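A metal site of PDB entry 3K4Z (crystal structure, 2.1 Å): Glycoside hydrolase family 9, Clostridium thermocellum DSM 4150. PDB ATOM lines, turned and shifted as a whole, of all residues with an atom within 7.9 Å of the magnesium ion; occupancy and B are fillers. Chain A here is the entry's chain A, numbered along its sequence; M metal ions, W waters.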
ATOM      1  N   GLU A  19     -17.863  11.108  29.217  1.00  0.00           N
ATOM      2  CA  GLU A  19     -18.520  10.766  27.957  1.00  0.00           C
ATOM      3  C   GLU A  19     -17.457  10.351  26.942  1.00  0.00           C
ATOM      4  O   GLU A  19     -16.505  11.077  26.718  1.00  0.00           O
ATOM      5  CB  GLU A  19     -19.326  11.928  27.444  1.00  0.00           C
ATOM      6  CG  GLU A  19     -20.224  11.601  26.177  1.00  0.00           C
ATOM      7  CD  GLU A  19     -21.105  10.428  26.366  1.00  0.00           C
ATOM      8  OE1 GLU A  19     -21.793  10.363  27.399  1.00  0.00           O
ATOM      9  OE2 GLU A  19     -21.118   9.542  25.509  1.00  0.00           O
ATOM     10  N   ARG A  20     -17.652   9.201  26.339  1.00  0.00           N
ATOM     11  CA  ARG A  20     -16.666   8.587  25.444  1.00  0.00           C
ATOM     12  C   ARG A  20     -17.242   8.217  24.109  1.00  0.00           C
ATOM     13  O   ARG A  20     -16.552   8.308  23.088  1.00  0.00           O
ATOM     14  CB  ARG A  20     -16.161   7.303  26.115  1.00  0.00           C
ATOM     15  CG  ARG A  20     -15.780   7.546  27.537  1.00  0.00           C
ATOM     16  CD  ARG A  20     -15.008   6.361  28.151  1.00  0.00           C
ATOM     17  NE  ARG A  20     -15.763   5.122  28.152  1.00  0.00           N
ATOM     18  CZ  ARG A  20     -15.272   3.938  28.482  1.00  0.00           C
ATOM     19  NH1 ARG A  20     -14.020   3.820  28.830  1.00  0.00           N
ATOM     20  NH2 ARG A  20     -16.034   2.851  28.470  1.00  0.00           N
ATOM     21  N   THR A  21     -18.486   7.751  24.098  1.00  0.00           N
ATOM     22  CA  THR A  21     -19.066   7.207  22.887  1.00  0.00           C
ATOM     23  C   THR A  21     -19.958   8.156  22.122  1.00  0.00           C
ATOM     24  O   THR A  21     -20.077   8.024  20.889  1.00  0.00           O
ATOM     25  CB  THR A  21     -19.894   5.925  23.129  1.00  0.00           C
ATOM     26  OG1 THR A  21     -21.060   6.272  23.830  1.00  0.00           O
ATOM     27  CG2 THR A  21     -19.088   4.788  23.906  1.00  0.00           C
ATOM     28  N   PHE A  22     -20.637   9.047  22.846  1.00  0.00           N
ATOM     29  CA  PHE A  22     -21.714   9.892  22.318  1.00  0.00           C
ATOM     30  C   PHE A  22     -22.944   9.213  21.724  1.00  0.00           C
ATOM     31  O   PHE A  22     -23.806   9.901  21.119  1.00  0.00           O
ATOM     32  CB  PHE A  22     -21.144  10.863  21.279  1.00  0.00           C
ATOM     33  CG  PHE A  22     -19.896  11.570  21.750  1.00  0.00           C
ATOM     34  CD1 PHE A  22     -19.984  12.611  22.643  1.00  0.00           C
ATOM     35  CD2 PHE A  22     -18.649  11.140  21.346  1.00  0.00           C
ATOM     36  CE1 PHE A  22     -18.860  13.242  23.073  1.00  0.00           C
ATOM     37  CE2 PHE A  22     -17.517  11.768  21.787  1.00  0.00           C
ATOM     38  CZ  PHE A  22     -17.630  12.820  22.656  1.00  0.00           C
ATOM     39  N   ASP A  23     -23.075   7.895  21.910  1.00  0.00           N
ATOM     40  CA  ASP A  23     -24.082   7.096  21.134  1.00  0.00           C
ATOM     41  C   ASP A  23     -25.498   7.303  21.613  1.00  0.00           C
ATOM     42  O   ASP A  23     -26.482   7.063  20.882  1.00  0.00           O
ATOM     43  CB  ASP A  23     -23.691   5.609  21.166  1.00  0.00           C
ATOM     44  CG  ASP A  23     -22.366   5.366  20.426  1.00  0.00           C
ATOM     45  OD1 ASP A  23     -21.916   6.242  19.684  1.00  0.00           O
ATOM     46  OD2 ASP A  23     -21.741   4.335  20.566  1.00  0.00           O
ATOM     47  N   GLU A  24     -25.637   7.832  22.822  1.00  0.00           N
ATOM     48  CA  GLU A  24     -26.960   8.189  23.310  1.00  0.00           C
ATOM     49  C   GLU A  24     -27.420   9.590  22.855  1.00  0.00           C
ATOM     50  O   GLU A  24     -28.542  10.034  23.215  1.00  0.00           O
ATOM     51  CB  GLU A  24     -26.983   8.052  24.829  1.00  0.00           C
ATOM     52  CG  GLU A  24     -26.676   6.627  25.311  1.00  0.00           C
ATOM     53  CD  GLU A  24     -25.152   6.240  25.292  1.00  0.00           C
ATOM     54  OE1 GLU A  24     -24.278   7.102  25.663  1.00  0.00           O
ATOM     55  OE2 GLU A  24     -24.847   5.059  24.921  1.00  0.00           O
ATOM     56  N   VAL A  44     -24.225  16.441  18.277  1.00  0.00           N
ATOM     57  CA  VAL A  44     -23.938  14.992  18.234  1.00  0.00           C
ATOM     58  C   VAL A  44     -24.712  14.421  17.071  1.00  0.00           C
ATOM     59  O   VAL A  44     -25.930  14.586  17.011  1.00  0.00           O
ATOM     60  CB  VAL A  44     -24.347  14.373  19.536  1.00  0.00           C
ATOM     61  CG1 VAL A  44     -24.144  12.813  19.556  1.00  0.00           C
ATOM     62  CG2 VAL A  44     -23.573  15.109  20.620  1.00  0.00           C
ATOM     63  N   VAL A  45     -24.029  13.761  16.155  1.00  0.00           N
ATOM     64  CA  VAL A  45     -24.644  13.251  14.934  1.00  0.00           C
ATOM     65  C   VAL A  45     -24.277  11.833  14.580  1.00  0.00           C
ATOM     66  O   VAL A  45     -23.231  11.338  14.995  1.00  0.00           O
ATOM     67  CB  VAL A  45     -24.232  14.144  13.770  1.00  0.00           C
ATOM     68  CG1 VAL A  45     -24.508  15.668  14.187  1.00  0.00           C
ATOM     69  CG2 VAL A  45     -22.825  13.956  13.462  1.00  0.00           C
ATOM     70  N   VAL A  47     -22.913   8.741  12.454  1.00  0.00           N
ATOM     71  CA  VAL A  47     -21.760   8.574  11.607  1.00  0.00           C
ATOM     72  C   VAL A  47     -22.086   7.667  10.442  1.00  0.00           C
ATOM     73  O   VAL A  47     -22.290   6.464  10.635  1.00  0.00           O
ATOM     74  CB  VAL A  47     -20.539   8.007  12.367  1.00  0.00           C
ATOM     75  CG1 VAL A  47     -19.333   7.888  11.465  1.00  0.00           C
ATOM     76  CG2 VAL A  47     -20.165   8.898  13.548  1.00  0.00           C
ATOM     77  N   GLN A  50     -21.368   3.732   9.921  1.00  0.00           N
ATOM     78  CA  GLN A  50     -21.222   3.120  11.237  1.00  0.00           C
ATOM     79  C   GLN A  50     -22.584   3.143  11.947  1.00  0.00           C
ATOM     80  O   GLN A  50     -22.799   3.914  12.855  1.00  0.00           O
ATOM     81  CB  GLN A  50     -20.107   3.847  12.024  1.00  0.00           C
ATOM     82  CG  GLN A  50     -18.723   3.718  11.345  1.00  0.00           C
ATOM     83  CD  GLN A  50     -17.624   4.421  12.139  1.00  0.00           C
ATOM     84  OE1 GLN A  50     -17.668   4.462  13.356  1.00  0.00           O
ATOM     85  NE2 GLN A  50     -16.668   5.010  11.444  1.00  0.00           N
ATOM     86  N   GLY A  52     -25.688   2.954  14.297  1.00  0.00           N
ATOM     87  CA  GLY A  52     -25.744   2.971  15.750  1.00  0.00           C
ATOM     88  C   GLY A  52     -24.745   3.926  16.397  1.00  0.00           C
ATOM     89  O   GLY A  52     -24.881   4.250  17.593  1.00  0.00           O
ATOM     90  N   ASN A  53     -23.708   4.346  15.659  1.00  0.00           N
ATOM     91  CA  ASN A  53     -22.664   5.123  16.233  1.00  0.00           C
ATOM     92  C   ASN A  53     -22.923   6.573  15.953  1.00  0.00           C
ATOM     93  O   ASN A  53     -23.166   6.912  14.799  1.00  0.00           O
ATOM     94  CB  ASN A  53     -21.301   4.757  15.633  1.00  0.00           C
ATOM     95  CG  ASN A  53     -20.175   5.354  16.428  1.00  0.00           C
ATOM     96  OD1 ASN A  53     -20.384   6.283  17.206  1.00  0.00           O
ATOM     97  ND2 ASN A  53     -18.983   4.759  16.321  1.00  0.00           N
ATOM     98  N   LYS A  54     -22.850   7.387  17.007  1.00  0.00           N
ATOM     99  CA  LYS A  54     -22.825   8.832  16.919  1.00  0.00           C
ATOM    100  C   LYS A  54     -21.480   9.411  17.397  1.00  0.00           C
ATOM    101  O   LYS A  54     -20.755   8.754  18.127  1.00  0.00           O
ATOM    102  CB  LYS A  54     -23.940   9.429  17.745  1.00  0.00           C
ATOM    103  CG  LYS A  54     -25.327   9.193  17.186  1.00  0.00           C
ATOM    104  CD  LYS A  54     -26.410   9.667  18.184  1.00  0.00           C
ATOM    105  CE  LYS A  54     -27.732   8.964  17.857  1.00  0.00           C
ATOM    106  NZ  LYS A  54     -28.401   9.656  16.773  1.00  0.00           N
ATOM    107  N   ALA A  55     -21.160  10.613  16.913  1.00  0.00           N
ATOM    108  CA  ALA A  55     -19.871  11.309  17.138  1.00  0.00           C
ATOM    109  C   ALA A  55     -20.161  12.720  17.567  1.00  0.00           C
ATOM    110  O   ALA A  55     -21.177  13.292  17.193  1.00  0.00           O
ATOM    111  CB  ALA A  55     -18.967  11.320  15.872  1.00  0.00           C
ATOM    112  N   PHE A  56     -19.337  13.231  18.467  1.00  0.00           N
ATOM    113  CA  PHE A  56     -19.271  14.668  18.756  1.00  0.00           C
ATOM    114  C   PHE A  56     -18.752  15.369  17.525  1.00  0.00           C
ATOM    115  O   PHE A  56     -17.696  15.043  17.025  1.00  0.00           O
ATOM    116  CB  PHE A  56     -18.386  14.901  19.967  1.00  0.00           C
ATOM    117  CG  PHE A  56     -18.405  16.331  20.550  1.00  0.00           C
ATOM    118  CD1 PHE A  56     -19.536  16.929  20.906  1.00  0.00           C
ATOM    119  CD2 PHE A  56     -17.230  16.986  20.796  1.00  0.00           C
ATOM    120  CE1 PHE A  56     -19.518  18.267  21.432  1.00  0.00           C
ATOM    121  CE2 PHE A  56     -17.190  18.236  21.285  1.00  0.00           C
ATOM    122  CZ  PHE A  56     -18.340  18.893  21.625  1.00  0.00           C
ATOM    123  N   LYS A  90     -10.827   8.294  18.164  1.00  0.00           N
ATOM    124  CA  LYS A  90     -10.949   8.343  16.731  1.00  0.00           C
ATOM    125  C   LYS A  90     -11.385   9.762  16.396  1.00  0.00           C
ATOM    126  O   LYS A  90     -12.328  10.273  16.988  1.00  0.00           O
ATOM    127  CB  LYS A  90     -11.963   7.321  16.250  1.00  0.00           C
ATOM    128  CG  LYS A  90     -11.386   5.911  16.261  1.00  0.00           C
ATOM    129  CD  LYS A  90     -12.395   4.801  15.961  1.00  0.00           C
ATOM    130  CE  LYS A  90     -13.425   4.717  17.019  1.00  0.00           C
ATOM    131  NZ  LYS A  90     -14.400   3.542  16.884  1.00  0.00           N
ATOM    132  N   TRP A  92     -11.667  12.599  12.824  1.00  0.00           N
ATOM    133  CA  TRP A  92     -11.661  12.809  11.388  1.00  0.00           C
ATOM    134  C   TRP A  92     -12.371  14.118  11.051  1.00  0.00           C
ATOM    135  O   TRP A  92     -12.999  14.741  11.926  1.00  0.00           O
ATOM    136  CB  TRP A  92     -12.223  11.581  10.627  1.00  0.00           C
ATOM    137  CG  TRP A  92     -13.722  11.358  10.803  1.00  0.00           C
ATOM    138  CD1 TRP A  92     -14.705  11.713   9.920  1.00  0.00           C
ATOM    139  CD2 TRP A  92     -14.379  10.744  11.915  1.00  0.00           C
ATOM    140  NE1 TRP A  92     -15.951  11.305  10.413  1.00  0.00           N
ATOM    141  CE2 TRP A  92     -15.763  10.713  11.640  1.00  0.00           C
ATOM    142  CE3 TRP A  92     -13.924  10.181  13.104  1.00  0.00           C
ATOM    143  CZ2 TRP A  92     -16.684  10.183  12.537  1.00  0.00           C
ATOM    144  CZ3 TRP A  92     -14.854   9.620  14.000  1.00  0.00           C
ATOM    145  CH2 TRP A  92     -16.218   9.628  13.693  1.00  0.00           C
ATOM    146  N   LEU A 165     -15.390  13.555  16.668  1.00  0.00           N
ATOM    147  CA  LEU A 165     -14.685  12.858  17.733  1.00  0.00           C
ATOM    148  C   LEU A 165     -15.543  11.689  18.254  1.00  0.00           C
ATOM    149  O   LEU A 165     -16.741  11.869  18.514  1.00  0.00           O
ATOM    150  CB  LEU A 165     -14.375  13.812  18.894  1.00  0.00           C
ATOM    151  CG  LEU A 165     -13.584  13.186  20.064  1.00  0.00           C
ATOM    152  CD1 LEU A 165     -12.179  12.802  19.678  1.00  0.00           C
ATOM    153  CD2 LEU A 165     -13.566  14.119  21.229  1.00  0.00           C
ATOM    154  N   ASP A 166     -14.899  10.567  18.557  1.00  0.00           N
ATOM    155  CA  ASP A 166     -15.607   9.325  18.924  1.00  0.00           C
ATOM    156  C   ASP A 166     -14.706   8.362  19.661  1.00  0.00           C
ATOM    157  O   ASP A 166     -13.473   8.348  19.458  1.00  0.00           O
ATOM    158  CB  ASP A 166     -16.208   8.660  17.675  1.00  0.00           C
ATOM    159  CG  ASP A 166     -17.179   7.571  17.984  1.00  0.00           C
ATOM    160  OD1 ASP A 166     -18.008   7.726  18.921  1.00  0.00           O
ATOM    161  OD2 ASP A 166     -17.115   6.546  17.263  1.00  0.00           O
ATOM    162  N   ASP A 167     -15.325   7.571  20.554  1.00  0.00           N
ATOM    163  CA  ASP A 167     -14.658   6.522  21.345  1.00  0.00           C
ATOM    164  C   ASP A 167     -13.397   7.084  21.953  1.00  0.00           C
ATOM    165  O   ASP A 167     -12.298   6.581  21.766  1.00  0.00           O
ATOM    166  CB  ASP A 167     -14.376   5.305  20.485  1.00  0.00           C
ATOM    167  CG  ASP A 167     -15.658   4.530  20.085  1.00  0.00           C
ATOM    168  OD1 ASP A 167     -16.740   4.697  20.756  1.00  0.00           O
ATOM    169  OD2 ASP A 167     -15.556   3.736  19.130  1.00  0.00           O
ATOM    170  N   VAL A 168     -13.594   8.165  22.677  1.00  0.00           N
ATOM    171  CA  VAL A 168     -12.488   8.918  23.228  1.00  0.00           C
ATOM    172  C   VAL A 168     -12.355   8.471  24.652  1.00  0.00           C
ATOM    173  O   VAL A 168     -13.334   8.382  25.377  1.00  0.00           O
ATOM    174  CB  VAL A 168     -12.669  10.454  23.132  1.00  0.00           C
ATOM    175  CG1 VAL A 168     -14.003  10.934  23.719  1.00  0.00           C
ATOM    176  CG2 VAL A 168     -11.451  11.159  23.874  1.00  0.00           C
HETATM  177 MG    MG M   1     -19.982   7.024  19.108  1.00  0.00          MG
HETATM  178  O   HOH W   1     -19.203   5.281  19.886  1.00  0.00           O
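Water W1 lies within hydrogen-bond range of the side-chain carboxylate of Asp 167 (2.7 Å) and the side-chain carboxylate of Asp 23 (2.8 Å).
The magnesium ion is bound by the backbone carbonyl oxygen (O) of Thr 21 (2.0 Å), water W1 (2.1 Å), the side-chain amide oxygen (OD1) of Asn 53 (2.1 Å), the side-chain carboxylate (OD1) of Asp 166 (2.1 Å), the backbone carbonyl oxygen (O) of Lys 54 (2.1 Å) and the side-chain carboxylate (OD1) of Asp 23 (2.2 Å).
The backbone NH (N) of Thr 21 sits at hydrogen-bond distance from the side-chain carboxylate (OE2) of Glu 19 (3.5 Å).
O of Asn 53 is in hydrogen-bond range of N of Val 47 (3.0 Å).
ND2 of Asn 53 is in hydrogen-bond range of OE1 of Gln 50 (3.3 Å).
The backbone carbonyl oxygen (O) of Asp 166 sits at hydrogen-bond distance from the backbone NH (N) of Lys 90, at 2.9 Å.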
